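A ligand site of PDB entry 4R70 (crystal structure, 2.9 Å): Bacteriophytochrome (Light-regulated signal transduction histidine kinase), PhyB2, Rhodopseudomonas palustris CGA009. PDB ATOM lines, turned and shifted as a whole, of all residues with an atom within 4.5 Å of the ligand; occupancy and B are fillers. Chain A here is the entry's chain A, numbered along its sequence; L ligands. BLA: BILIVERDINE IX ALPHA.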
ATOM      1  N   CYS A  28      17.465  -0.583  20.746  1.00  0.00           N
ATOM      2  CA  CYS A  28      18.595  -0.194  19.850  1.00  0.00           C
ATOM      3  C   CYS A  28      19.132   1.117  20.342  1.00  0.00           C
ATOM      4  O   CYS A  28      20.345   1.312  20.365  1.00  0.00           O
ATOM      5  CB  CYS A  28      18.198  -0.022  18.353  1.00  0.00           C
ATOM      6  SG  CYS A  28      18.612  -1.375  17.211  1.00  0.00           S
ATOM      7  N   GLU A  31      21.629   1.081  23.853  1.00  0.00           N
ATOM      8  CA  GLU A  31      22.997   0.572  23.944  1.00  0.00           C
ATOM      9  C   GLU A  31      23.902   1.747  24.155  1.00  0.00           C
ATOM     10  O   GLU A  31      23.923   2.664  23.292  1.00  0.00           O
ATOM     11  CB  GLU A  31      23.406  -0.221  22.714  1.00  0.00           C
ATOM     12  CG  GLU A  31      24.873  -0.628  22.741  1.00  0.00           C
ATOM     13  CD  GLU A  31      25.297  -1.409  21.486  1.00  0.00           C
ATOM     14  OE1 GLU A  31      24.431  -1.527  20.582  1.00  0.00           O
ATOM     15  OE2 GLU A  31      26.481  -1.870  21.390  1.00  0.00           O
ATOM     16  N   ILE A  33      27.159   3.661  24.071  1.00  0.00           N
ATOM     17  CA  ILE A  33      28.311   3.354  23.251  1.00  0.00           C
ATOM     18  C   ILE A  33      29.564   4.069  23.710  1.00  0.00           C
ATOM     19  O   ILE A  33      30.654   3.868  23.161  1.00  0.00           O
ATOM     20  CB  ILE A  33      28.063   3.682  21.785  1.00  0.00           C
ATOM     21  CG1 ILE A  33      27.928   5.164  21.577  1.00  0.00           C
ATOM     22  CG2 ILE A  33      26.821   2.922  21.236  1.00  0.00           C
ATOM     23  CD1 ILE A  33      27.388   5.454  20.191  1.00  0.00           C
ATOM     24  N   LYS A 183      29.647   8.749   0.324  1.00  0.00           N
ATOM     25  CA  LYS A 183      28.231   9.025   0.221  1.00  0.00           C
ATOM     26  C   LYS A 183      27.839  10.275   0.937  1.00  0.00           C
ATOM     27  O   LYS A 183      28.389  10.560   2.005  1.00  0.00           O
ATOM     28  CB  LYS A 183      27.491   7.859   0.832  1.00  0.00           C
ATOM     29  CG  LYS A 183      27.568   6.616  -0.038  1.00  0.00           C
ATOM     30  CD  LYS A 183      27.313   5.324   0.752  1.00  0.00           C
ATOM     31  CE  LYS A 183      28.370   5.122   1.834  1.00  0.00           C
ATOM     32  NZ  LYS A 183      29.628   4.883   1.115  1.00  0.00           N
ATOM     33  N   TYR A 185      24.704  11.556   2.916  1.00  0.00           N
ATOM     34  CA  TYR A 185      23.442  11.048   3.433  1.00  0.00           C
ATOM     35  C   TYR A 185      22.645  12.071   4.188  1.00  0.00           C
ATOM     36  O   TYR A 185      23.089  12.599   5.268  1.00  0.00           O
ATOM     37  CB  TYR A 185      23.734   9.978   4.433  1.00  0.00           C
ATOM     38  CG  TYR A 185      22.532   9.251   4.981  1.00  0.00           C
ATOM     39  CD1 TYR A 185      21.791   8.406   4.196  1.00  0.00           C
ATOM     40  CD2 TYR A 185      22.202   9.297   6.348  1.00  0.00           C
ATOM     41  CE1 TYR A 185      20.739   7.654   4.742  1.00  0.00           C
ATOM     42  CE2 TYR A 185      21.127   8.549   6.903  1.00  0.00           C
ATOM     43  CZ  TYR A 185      20.412   7.710   6.065  1.00  0.00           C
ATOM     44  OH  TYR A 185      19.359   6.937   6.539  1.00  0.00           O
ATOM     45  N   VAL A 195      20.689   8.532   0.555  1.00  0.00           N
ATOM     46  CA  VAL A 195      21.940   8.957  -0.038  1.00  0.00           C
ATOM     47  C   VAL A 195      21.627   9.928  -1.159  1.00  0.00           C
ATOM     48  O   VAL A 195      21.130   9.509  -2.182  1.00  0.00           O
ATOM     49  CB  VAL A 195      22.625   7.697  -0.655  1.00  0.00           C
ATOM     50  CG1 VAL A 195      23.803   8.019  -1.506  1.00  0.00           C
ATOM     51  CG2 VAL A 195      23.111   6.867   0.424  1.00  0.00           C
ATOM     52  N   LEU A 207      24.853   2.740  -3.874  1.00  0.00           N
ATOM     53  CA  LEU A 207      23.682   2.979  -3.092  1.00  0.00           C
ATOM     54  C   LEU A 207      23.075   4.358  -3.281  1.00  0.00           C
ATOM     55  O   LEU A 207      22.561   4.921  -2.333  1.00  0.00           O
ATOM     56  CB  LEU A 207      23.975   2.790  -1.626  1.00  0.00           C
ATOM     57  CG  LEU A 207      23.840   1.458  -0.946  1.00  0.00           C
ATOM     58  CD1 LEU A 207      24.193   0.446  -1.917  1.00  0.00           C
ATOM     59  CD2 LEU A 207      24.879   1.619  -0.029  1.00  0.00           C
ATOM     60  N   PHE A 212      17.123   4.650   4.058  1.00  0.00           N
ATOM     61  CA  PHE A 212      17.553   3.775   5.130  1.00  0.00           C
ATOM     62  C   PHE A 212      16.709   4.094   6.339  1.00  0.00           C
ATOM     63  O   PHE A 212      16.293   5.236   6.553  1.00  0.00           O
ATOM     64  CB  PHE A 212      19.065   3.968   5.442  1.00  0.00           C
ATOM     65  CG  PHE A 212      19.978   3.309   4.440  1.00  0.00           C
ATOM     66  CD1 PHE A 212      20.222   3.877   3.192  1.00  0.00           C
ATOM     67  CD2 PHE A 212      20.612   2.129   4.755  1.00  0.00           C
ATOM     68  CE1 PHE A 212      21.051   3.244   2.246  1.00  0.00           C
ATOM     69  CE2 PHE A 212      21.419   1.491   3.839  1.00  0.00           C
ATOM     70  CZ  PHE A 212      21.636   2.067   2.585  1.00  0.00           C
ATOM     71  N   SER A 215      16.463   3.259  12.375  1.00  0.00           N
ATOM     72  CA  SER A 215      17.099   2.244  13.151  1.00  0.00           C
ATOM     73  C   SER A 215      18.625   2.279  12.876  1.00  0.00           C
ATOM     74  O   SER A 215      19.441   2.016  13.751  1.00  0.00           O
ATOM     75  CB  SER A 215      16.454   0.886  12.822  1.00  0.00           C
ATOM     76  OG  SER A 215      17.385  -0.207  12.769  1.00  0.00           O
ATOM     77  N   ASP A 216      19.037   2.683  11.681  1.00  0.00           N
ATOM     78  CA  ASP A 216      20.409   2.364  11.287  1.00  0.00           C
ATOM     79  C   ASP A 216      21.402   3.297  11.963  1.00  0.00           C
ATOM     80  O   ASP A 216      22.536   2.929  12.215  1.00  0.00           O
ATOM     81  CB  ASP A 216      20.596   2.426   9.801  1.00  0.00           C
ATOM     82  CG  ASP A 216      19.912   1.298   9.086  1.00  0.00           C
ATOM     83  OD1 ASP A 216      18.997   0.705   9.661  1.00  0.00           O
ATOM     84  OD2 ASP A 216      20.249   1.031   7.920  1.00  0.00           O
ATOM     85  N   ILE A 217      20.966   4.514  12.246  1.00  0.00           N
ATOM     86  CA  ILE A 217      21.733   5.362  13.099  1.00  0.00           C
ATOM     87  C   ILE A 217      20.758   5.788  14.123  1.00  0.00           C
ATOM     88  O   ILE A 217      20.030   6.749  13.914  1.00  0.00           O
ATOM     89  CB  ILE A 217      22.221   6.532  12.359  1.00  0.00           C
ATOM     90  CG1 ILE A 217      23.203   6.045  11.327  1.00  0.00           C
ATOM     91  CG2 ILE A 217      22.964   7.384  13.275  1.00  0.00           C
ATOM     92  CD1 ILE A 217      23.361   6.973  10.170  1.00  0.00           C
ATOM     93  N   PRO A 218      20.718   5.041  15.235  1.00  0.00           N
ATOM     94  CA  PRO A 218      19.807   5.025  16.377  1.00  0.00           C
ATOM     95  C   PRO A 218      20.023   6.292  17.139  1.00  0.00           C
ATOM     96  O   PRO A 218      21.037   6.931  16.839  1.00  0.00           O
ATOM     97  CB  PRO A 218      20.316   3.885  17.213  1.00  0.00           C
ATOM     98  CG  PRO A 218      21.672   3.613  16.728  1.00  0.00           C
ATOM     99  CD  PRO A 218      21.798   4.064  15.371  1.00  0.00           C
ATOM    100  N   GLN A 220      20.908   7.649  20.097  1.00  0.00           N
ATOM    101  CA  GLN A 220      22.117   7.958  20.839  1.00  0.00           C
ATOM    102  C   GLN A 220      23.266   8.169  19.936  1.00  0.00           C
ATOM    103  O   GLN A 220      24.049   9.060  20.170  1.00  0.00           O
ATOM    104  CB  GLN A 220      22.405   6.872  21.920  1.00  0.00           C
ATOM    105  CG  GLN A 220      22.940   5.536  21.396  1.00  0.00           C
ATOM    106  CD  GLN A 220      22.020   4.889  20.333  1.00  0.00           C
ATOM    107  OE1 GLN A 220      21.091   5.514  19.750  1.00  0.00           O
ATOM    108  NE2 GLN A 220      22.290   3.627  20.080  1.00  0.00           N
ATOM    109  N   SER A 221      23.374   7.370  18.880  1.00  0.00           N
ATOM    110  CA  SER A 221      24.411   7.618  17.908  1.00  0.00           C
ATOM    111  C   SER A 221      24.323   9.046  17.384  1.00  0.00           C
ATOM    112  O   SER A 221      25.307   9.786  17.419  1.00  0.00           O
ATOM    113  CB  SER A 221      24.298   6.636  16.755  1.00  0.00           C
ATOM    114  OG  SER A 221      24.460   5.324  17.257  1.00  0.00           O
ATOM    115  N   TYR A 225      26.923  12.033  17.464  1.00  0.00           N
ATOM    116  CA  TYR A 225      27.384  12.606  16.213  1.00  0.00           C
ATOM    117  C   TYR A 225      27.000  14.070  16.122  1.00  0.00           C
ATOM    118  O   TYR A 225      27.506  14.802  15.302  1.00  0.00           O
ATOM    119  CB  TYR A 225      26.921  11.804  14.973  1.00  0.00           C
ATOM    120  CG  TYR A 225      27.361  10.365  15.081  1.00  0.00           C
ATOM    121  CD1 TYR A 225      28.494  10.034  15.821  1.00  0.00           C
ATOM    122  CD2 TYR A 225      26.616   9.343  14.501  1.00  0.00           C
ATOM    123  CE1 TYR A 225      28.897   8.725  15.971  1.00  0.00           C
ATOM    124  CE2 TYR A 225      27.000   8.031  14.626  1.00  0.00           C
ATOM    125  CZ  TYR A 225      28.133   7.699  15.366  1.00  0.00           C
ATOM    126  OH  TYR A 225      28.459   6.331  15.474  1.00  0.00           O
ATOM    127  N   ARG A 231      34.351  10.476  13.027  1.00  0.00           N
ATOM    128  CA  ARG A 231      34.726   9.197  13.633  1.00  0.00           C
ATOM    129  C   ARG A 231      35.241   8.294  12.519  1.00  0.00           C
ATOM    130  O   ARG A 231      34.892   8.500  11.348  1.00  0.00           O
ATOM    131  CB  ARG A 231      33.542   8.532  14.228  1.00  0.00           C
ATOM    132  CG  ARG A 231      32.587   8.217  13.173  1.00  0.00           C
ATOM    133  CD  ARG A 231      31.264   8.519  13.683  1.00  0.00           C
ATOM    134  NE  ARG A 231      31.182   9.939  13.970  1.00  0.00           N
ATOM    135  CZ  ARG A 231      30.444  10.756  13.245  1.00  0.00           C
ATOM    136  NH1 ARG A 231      30.370  12.038  13.513  1.00  0.00           N
ATOM    137  NH2 ARG A 231      29.779  10.258  12.236  1.00  0.00           N
ATOM    138  N   ILE A 233      36.680   4.069  11.715  1.00  0.00           N
ATOM    139  CA  ILE A 233      36.926   2.662  12.047  1.00  0.00           C
ATOM    140  C   ILE A 233      37.793   2.031  10.968  1.00  0.00           C
ATOM    141  O   ILE A 233      37.269   1.463  10.027  1.00  0.00           O
ATOM    142  CB  ILE A 233      35.633   1.965  12.017  1.00  0.00           C
ATOM    143  CG1 ILE A 233      34.654   2.795  12.819  1.00  0.00           C
ATOM    144  CG2 ILE A 233      35.809   0.489  12.508  1.00  0.00           C
ATOM    145  CD1 ILE A 233      33.308   2.194  12.986  1.00  0.00           C
ATOM    146  N   ARG A 263      37.867   5.353  20.294  1.00  0.00           N
ATOM    147  CA  ARG A 263      36.867   4.561  21.035  1.00  0.00           C
ATOM    148  C   ARG A 263      36.250   3.405  20.269  1.00  0.00           C
ATOM    149  O   ARG A 263      35.454   3.622  19.378  1.00  0.00           O
ATOM    150  CB  ARG A 263      35.755   5.497  21.486  1.00  0.00           C
ATOM    151  CG  ARG A 263      34.578   4.782  22.082  1.00  0.00           C
ATOM    152  CD  ARG A 263      33.345   5.680  22.147  1.00  0.00           C
ATOM    153  NE  ARG A 263      32.973   6.316  20.866  1.00  0.00           N
ATOM    154  CZ  ARG A 263      31.970   5.912  20.073  1.00  0.00           C
ATOM    155  NH1 ARG A 263      31.636   6.556  18.925  1.00  0.00           N
ATOM    156  NH2 ARG A 263      31.281   4.841  20.415  1.00  0.00           N
ATOM    157  N   VAL A 265      33.735   0.841  18.983  1.00  0.00           N
ATOM    158  CA  VAL A 265      32.367   1.282  18.779  1.00  0.00           C
ATOM    159  C   VAL A 265      31.468   0.165  19.104  1.00  0.00           C
ATOM    160  O   VAL A 265      31.942  -0.914  19.425  1.00  0.00           O
ATOM    161  CB  VAL A 265      32.053   1.629  17.300  1.00  0.00           C
ATOM    162  CG1 VAL A 265      32.916   2.811  16.781  1.00  0.00           C
ATOM    163  CG2 VAL A 265      32.229   0.459  16.452  1.00  0.00           C
ATOM    164  N   SER A 266      30.179   0.406  19.065  1.00  0.00           N
ATOM    165  CA  SER A 266      29.225  -0.706  19.150  1.00  0.00           C
ATOM    166  C   SER A 266      29.544  -1.881  18.246  1.00  0.00           C
ATOM    167  O   SER A 266      29.827  -1.711  17.072  1.00  0.00           O
ATOM    168  CB  SER A 266      27.813  -0.247  18.804  1.00  0.00           C
ATOM    169  OG  SER A 266      27.026  -1.366  18.483  1.00  0.00           O
ATOM    170  N   THR A 268      27.124  -4.051  17.434  1.00  0.00           N
ATOM    171  CA  THR A 268      25.980  -4.078  16.520  1.00  0.00           C
ATOM    172  C   THR A 268      26.361  -3.517  15.156  1.00  0.00           C
ATOM    173  O   THR A 268      26.187  -4.125  14.106  1.00  0.00           O
ATOM    174  CB  THR A 268      24.835  -3.226  17.025  1.00  0.00           C
ATOM    175  OG1 THR A 268      24.267  -3.876  18.164  1.00  0.00           O
ATOM    176  CG2 THR A 268      23.789  -3.107  15.958  1.00  0.00           C
ATOM    177  N   HIS A 269      26.913  -2.329  15.190  1.00  0.00           N
ATOM    178  CA  HIS A 269      27.258  -1.647  13.971  1.00  0.00           C
ATOM    179  C   HIS A 269      28.327  -2.382  13.190  1.00  0.00           C
ATOM    180  O   HIS A 269      28.305  -2.487  11.957  1.00  0.00           O
ATOM    181  CB  HIS A 269      27.797  -0.267  14.302  1.00  0.00           C
ATOM    182  CG  HIS A 269      28.161   0.546  13.106  1.00  0.00           C
ATOM    183  ND1 HIS A 269      27.273   0.796  12.107  1.00  0.00           N
ATOM    184  CD2 HIS A 269      29.282   1.214  12.791  1.00  0.00           C
ATOM    185  CE1 HIS A 269      27.830   1.594  11.186  1.00  0.00           C
ATOM    186  NE2 HIS A 269      29.054   1.865  11.610  1.00  0.00           N
ATOM    187  N   TYR A 272      26.919  -4.729  10.947  1.00  0.00           N
ATOM    188  CA  TYR A 272      26.297  -3.983   9.864  1.00  0.00           C
ATOM    189  C   TYR A 272      27.242  -3.880   8.715  1.00  0.00           C
ATOM    190  O   TYR A 272      26.916  -4.095   7.551  1.00  0.00           O
ATOM    191  CB  TYR A 272      25.967  -2.620  10.372  1.00  0.00           C
ATOM    192  CG  TYR A 272      25.186  -1.744   9.430  1.00  0.00           C
ATOM    193  CD1 TYR A 272      25.821  -0.797   8.683  1.00  0.00           C
ATOM    194  CD2 TYR A 272      23.818  -1.843   9.343  1.00  0.00           C
ATOM    195  CE1 TYR A 272      25.107   0.011   7.849  1.00  0.00           C
ATOM    196  CE2 TYR A 272      23.084  -1.024   8.510  1.00  0.00           C
ATOM    197  CZ  TYR A 272      23.734  -0.104   7.760  1.00  0.00           C
ATOM    198  OH  TYR A 272      23.020   0.723   6.915  1.00  0.00           O
ATOM    199  N   MET A 273      28.459  -3.588   9.085  1.00  0.00           N
ATOM    200  CA  MET A 273      29.475  -3.260   8.145  1.00  0.00           C
ATOM    201  C   MET A 273      30.049  -4.458   7.410  1.00  0.00           C
ATOM    202  O   MET A 273      30.219  -4.392   6.197  1.00  0.00           O
ATOM    203  CB  MET A 273      30.508  -2.485   8.895  1.00  0.00           C
ATOM    204  CG  MET A 273      29.913  -1.104   9.197  1.00  0.00           C
ATOM    205  SD  MET A 273      30.030  -0.059   7.738  1.00  0.00           S
ATOM    206  CE  MET A 273      28.541  -0.290   6.809  1.00  0.00           C
ATOM    207  N   ALA A 281      35.410   2.378   7.647  1.00  0.00           N
ATOM    208  CA  ALA A 281      34.335   3.347   7.645  1.00  0.00           C
ATOM    209  C   ALA A 281      34.793   4.599   8.317  1.00  0.00           C
ATOM    210  O   ALA A 281      35.379   4.509   9.381  1.00  0.00           O
ATOM    211  CB  ALA A 281      33.197   2.783   8.428  1.00  0.00           C
ATOM    212  N   MET A 282      34.491   5.760   7.736  1.00  0.00           N
ATOM    213  CA  MET A 282      34.756   7.057   8.352  1.00  0.00           C
ATOM    214  C   MET A 282      33.529   7.888   8.058  1.00  0.00           C
ATOM    215  O   MET A 282      32.971   7.819   6.964  1.00  0.00           O
ATOM    216  CB  MET A 282      35.932   7.747   7.720  1.00  0.00           C
ATOM    217  CG  MET A 282      36.448   8.796   8.587  1.00  0.00           C
ATOM    218  SD  MET A 282      37.447   9.915   7.614  1.00  0.00           S
ATOM    219  CE  MET A 282      38.634   8.781   6.927  1.00  0.00           C
ATOM    220  N   SER A 283      33.146   8.736   8.972  1.00  0.00           N
ATOM    221  CA  SER A 283      31.977   9.544   8.737  1.00  0.00           C
ATOM    222  C   SER A 283      32.099  10.915   9.356  1.00  0.00           C
ATOM    223  O   SER A 283      32.533  11.071  10.486  1.00  0.00           O
ATOM    224  CB  SER A 283      30.747   8.775   9.209  1.00  0.00           C
ATOM    225  OG  SER A 283      30.863   8.471  10.572  1.00  0.00           O
ATOM    226  N   SER A 297      29.424   9.680   4.680  1.00  0.00           N
ATOM    227  CA  SER A 297      29.906   8.408   5.116  1.00  0.00           C
ATOM    228  C   SER A 297      30.891   7.869   4.109  1.00  0.00           C
ATOM    229  O   SER A 297      30.602   7.836   2.896  1.00  0.00           O
ATOM    230  CB  SER A 297      28.781   7.405   5.251  1.00  0.00           C
ATOM    231  OG  SER A 297      29.349   6.176   5.607  1.00  0.00           O
ATOM    232  N   HIS A 299      33.351   4.666   2.866  1.00  0.00           N
ATOM    233  CA  HIS A 299      33.536   3.221   2.974  1.00  0.00           C
ATOM    234  C   HIS A 299      34.649   2.725   2.072  1.00  0.00           C
ATOM    235  O   HIS A 299      34.758   3.205   0.939  1.00  0.00           O
ATOM    236  CB  HIS A 299      32.216   2.506   2.682  1.00  0.00           C
ATOM    237  CG  HIS A 299      31.153   2.756   3.711  1.00  0.00           C
ATOM    238  ND1 HIS A 299      29.894   2.192   3.615  1.00  0.00           N
ATOM    239  CD2 HIS A 299      31.159   3.465   4.862  1.00  0.00           C
ATOM    240  CE1 HIS A 299      29.196   2.522   4.686  1.00  0.00           C
ATOM    241  NE2 HIS A 299      29.933   3.306   5.445  1.00  0.00           N
ATOM    242  N   PRO A 468      14.279  -4.369  10.155  1.00  0.00           N
ATOM    243  CA  PRO A 468      15.541  -3.603  10.135  1.00  0.00           C
ATOM    244  C   PRO A 468      16.628  -4.161  11.076  1.00  0.00           C
ATOM    245  O   PRO A 468      17.656  -3.503  11.323  1.00  0.00           O
ATOM    246  CB  PRO A 468      15.087  -2.188  10.581  1.00  0.00           C
ATOM    247  CG  PRO A 468      13.906  -2.437  11.479  1.00  0.00           C
ATOM    248  CD  PRO A 468      13.216  -3.685  10.907  1.00  0.00           C
ATOM    249  N   VAL A 469      16.380  -5.377  11.560  1.00  0.00           N
ATOM    250  CA  VAL A 469      17.220  -6.084  12.519  1.00  0.00           C
ATOM    251  C   VAL A 469      16.794  -7.539  12.530  1.00  0.00           C
ATOM    252  O   VAL A 469      15.830  -7.924  11.881  1.00  0.00           O
ATOM    253  CB  VAL A 469      16.954  -5.618  13.942  1.00  0.00           C
ATOM    254  CG1 VAL A 469      17.736  -4.370  14.248  1.00  0.00           C
ATOM    255  CG2 VAL A 469      15.456  -5.337  14.141  1.00  0.00           C
ATOM    256  N   THR A 480      22.323  -6.601  12.790  1.00  0.00           N
ATOM    257  CA  THR A 480      22.028  -5.940  11.534  1.00  0.00           C
ATOM    258  C   THR A 480      21.452  -6.962  10.541  1.00  0.00           C
ATOM    259  O   THR A 480      21.949  -8.074  10.429  1.00  0.00           O
ATOM    260  CB  THR A 480      23.305  -5.308  11.047  1.00  0.00           C
ATOM    261  OG1 THR A 480      24.256  -6.334  10.728  1.00  0.00           O
ATOM    262  CG2 THR A 480      23.859  -4.573  12.212  1.00  0.00           C
HETATM  263  CHA BLA L   1      26.997   3.845  13.698  1.00  0.00           C
HETATM  264  NA  BLA L   1      25.736   3.716  11.583  1.00  0.00           N
HETATM  265  C1A BLA L   1      26.741   4.136  12.348  1.00  0.00           C
HETATM  266  C2A BLA L   1      27.521   4.961  11.557  1.00  0.00           C
HETATM  267  C3A BLA L   1      26.871   4.983  10.324  1.00  0.00           C
HETATM  268  C4A BLA L   1      25.781   4.166  10.344  1.00  0.00           C
HETATM  269  CMA BLA L   1      27.348   5.823   9.156  1.00  0.00           C
HETATM  270  CAA BLA L   1      28.815   5.709  11.964  1.00  0.00           C
HETATM  271  CBA BLA L   1      30.139   4.967  11.546  1.00  0.00           C
HETATM  272  CGA BLA L   1      30.289   4.757  10.005  1.00  0.00           C
HETATM  273  O1A BLA L   1      30.046   3.598   9.572  1.00  0.00           O
HETATM  274  O2A BLA L   1      30.588   5.744   9.249  1.00  0.00           O
HETATM  275  CHB BLA L   1      24.679   3.855   9.369  1.00  0.00           C
HETATM  276  NB  BLA L   1      26.020   4.155   7.296  1.00  0.00           N
HETATM  277  C1B BLA L   1      24.858   4.099   7.925  1.00  0.00           C
HETATM  278  C2B BLA L   1      23.867   4.195   6.973  1.00  0.00           C
HETATM  279  C3B BLA L   1      24.463   4.279   5.745  1.00  0.00           C
HETATM  280  C4B BLA L   1      25.815   4.312   5.991  1.00  0.00           C
HETATM  281  CMB BLA L   1      22.372   4.104   7.157  1.00  0.00           C
HETATM  282  OB  BLA L   1      26.695   4.423   5.139  1.00  0.00           O
HETATM  283  CAB BLA L   1      23.772   4.360   4.546  1.00  0.00           C
HETATM  284  CBB BLA L   1      24.405   4.447   3.321  1.00  0.00           C
HETATM  285  NC  BLA L   1      22.731   0.248  13.174  1.00  0.00           N
HETATM  286  C1C BLA L   1      21.877  -0.540  12.529  1.00  0.00           C
HETATM  287  C2C BLA L   1      21.145  -1.235  13.424  1.00  0.00           C
HETATM  288  C3C BLA L   1      21.569  -0.882  14.678  1.00  0.00           C
HETATM  289  C4C BLA L   1      22.587   0.072  14.483  1.00  0.00           C
HETATM  290  CMC BLA L   1      20.064  -2.216  13.002  1.00  0.00           C
HETATM  291  OC  BLA L   1      21.688  -0.689  11.326  1.00  0.00           O
HETATM  292  CAC BLA L   1      20.975  -1.451  15.974  1.00  0.00           C
HETATM  293  CBC BLA L   1      19.817  -0.570  16.428  1.00  0.00           C
HETATM  294  CHD BLA L   1      23.370   0.771  15.603  1.00  0.00           C
HETATM  295  ND  BLA L   1      25.058   2.274  14.251  1.00  0.00           N
HETATM  296  C1D BLA L   1      24.569   1.733  15.366  1.00  0.00           C
HETATM  297  C2D BLA L   1      25.346   2.248  16.394  1.00  0.00           C
HETATM  298  C3D BLA L   1      26.337   3.046  15.847  1.00  0.00           C
HETATM  299  C4D BLA L   1      26.158   3.018  14.478  1.00  0.00           C
HETATM  300  CMD BLA L   1      25.164   1.938  17.877  1.00  0.00           C
HETATM  301  CAD BLA L   1      27.449   3.846  16.569  1.00  0.00           C
HETATM  302  CBD BLA L   1      28.580   3.037  17.106  1.00  0.00           C
HETATM  303  CGD BLA L   1      29.559   3.964  17.770  1.00  0.00           C
HETATM  304  O1D BLA L   1      29.984   3.474  18.853  1.00  0.00           O
HETATM  305  O2D BLA L   1      29.886   5.068  17.167  1.00  0.00           O
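A carbon (CBC) of the ligand is bonded to the side-chain sulfur of Cys 28. NH2 of Arg 263 is in salt-bridge range of O1D of the ligand, at 2.4 Å. The side-chain hydroxyl (OH) of Tyr 225 sits at hydrogen-bond distance from an oxygen (O2D) of the ligand, at 2.5 Å. NE2 of His 269 sits at hydrogen-bond distance from O1A of the ligand (2.9 Å). A nitrogen (NC) of the ligand sits at hydrogen-bond distance from the backbone carbonyl oxygen of Asp 216 (2.9 Å). The side-chain hydroxyl (OG) of Ser 283 sits close to an oxygen (O2A) of the ligand (3.0 Å). An oxygen (O1D) of the ligand lies within hydrogen-bond range of the backbone NH (N) of Ser 266, at 3.1 Å. A ring nitrogen (NE2) of His 299 lies close to an oxygen (OB) of the ligand, 3.4 Å away. The side-chain hydroxyl (OG) of Ser 297 is in hydrogen-bond range of an oxygen (OB) of the ligand, at 3.2 Å.
The backbone carbonyl oxygen (O) of Ile 33 lies within hydrogen-bond range of the guanidinium group (NH2) of Arg 263, at 3.0 Å. N of His 269 is in hydrogen-bond range of OG of Ser 266 (3.4 Å). The side-chain hydroxyl (OG) of Ser 283 lies within hydrogen-bond range of the guanidinium group (NH2) of Arg 231 (2.7 Å). The backbone NH (N) of Thr 268 lies within hydrogen-bond range of the side-chain hydroxyl (OG) of Ser 266, at 2.9 Å. OG of Ser 297 lies within hydrogen-bond range of NE2 of His 299 (2.9 Å). The backbone carbonyl oxygen (O) of Ser 297 is in hydrogen-bond range of the backbone NH (N) of Lys 183 (2.9 Å). O of Ala 281 is in hydrogen-bond range of N of Ile 233, 2.7 Å away. The backbone carbonyl oxygen of Pro 218 sits close to the side-chain amide oxygen of Gln 220.
Residues that only touch the ligand: Tyr 272, Val 265, Pro 468, Thr 268, Ser 221, Ile 217, Ser 215, Val 469, Ala 281, Pro 218, Ile 33, Phe 212, Lys 183, Met 282, Val 195 and Gln 220. Hydrophobic or aromatic side chains within 4 Å of the ligand: Ile 33, Val 195, Phe 212, Ile 217, Pro 218, Tyr 225, Val 265, His 269, Tyr 272, Ala 281, His 299 and Val 469.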
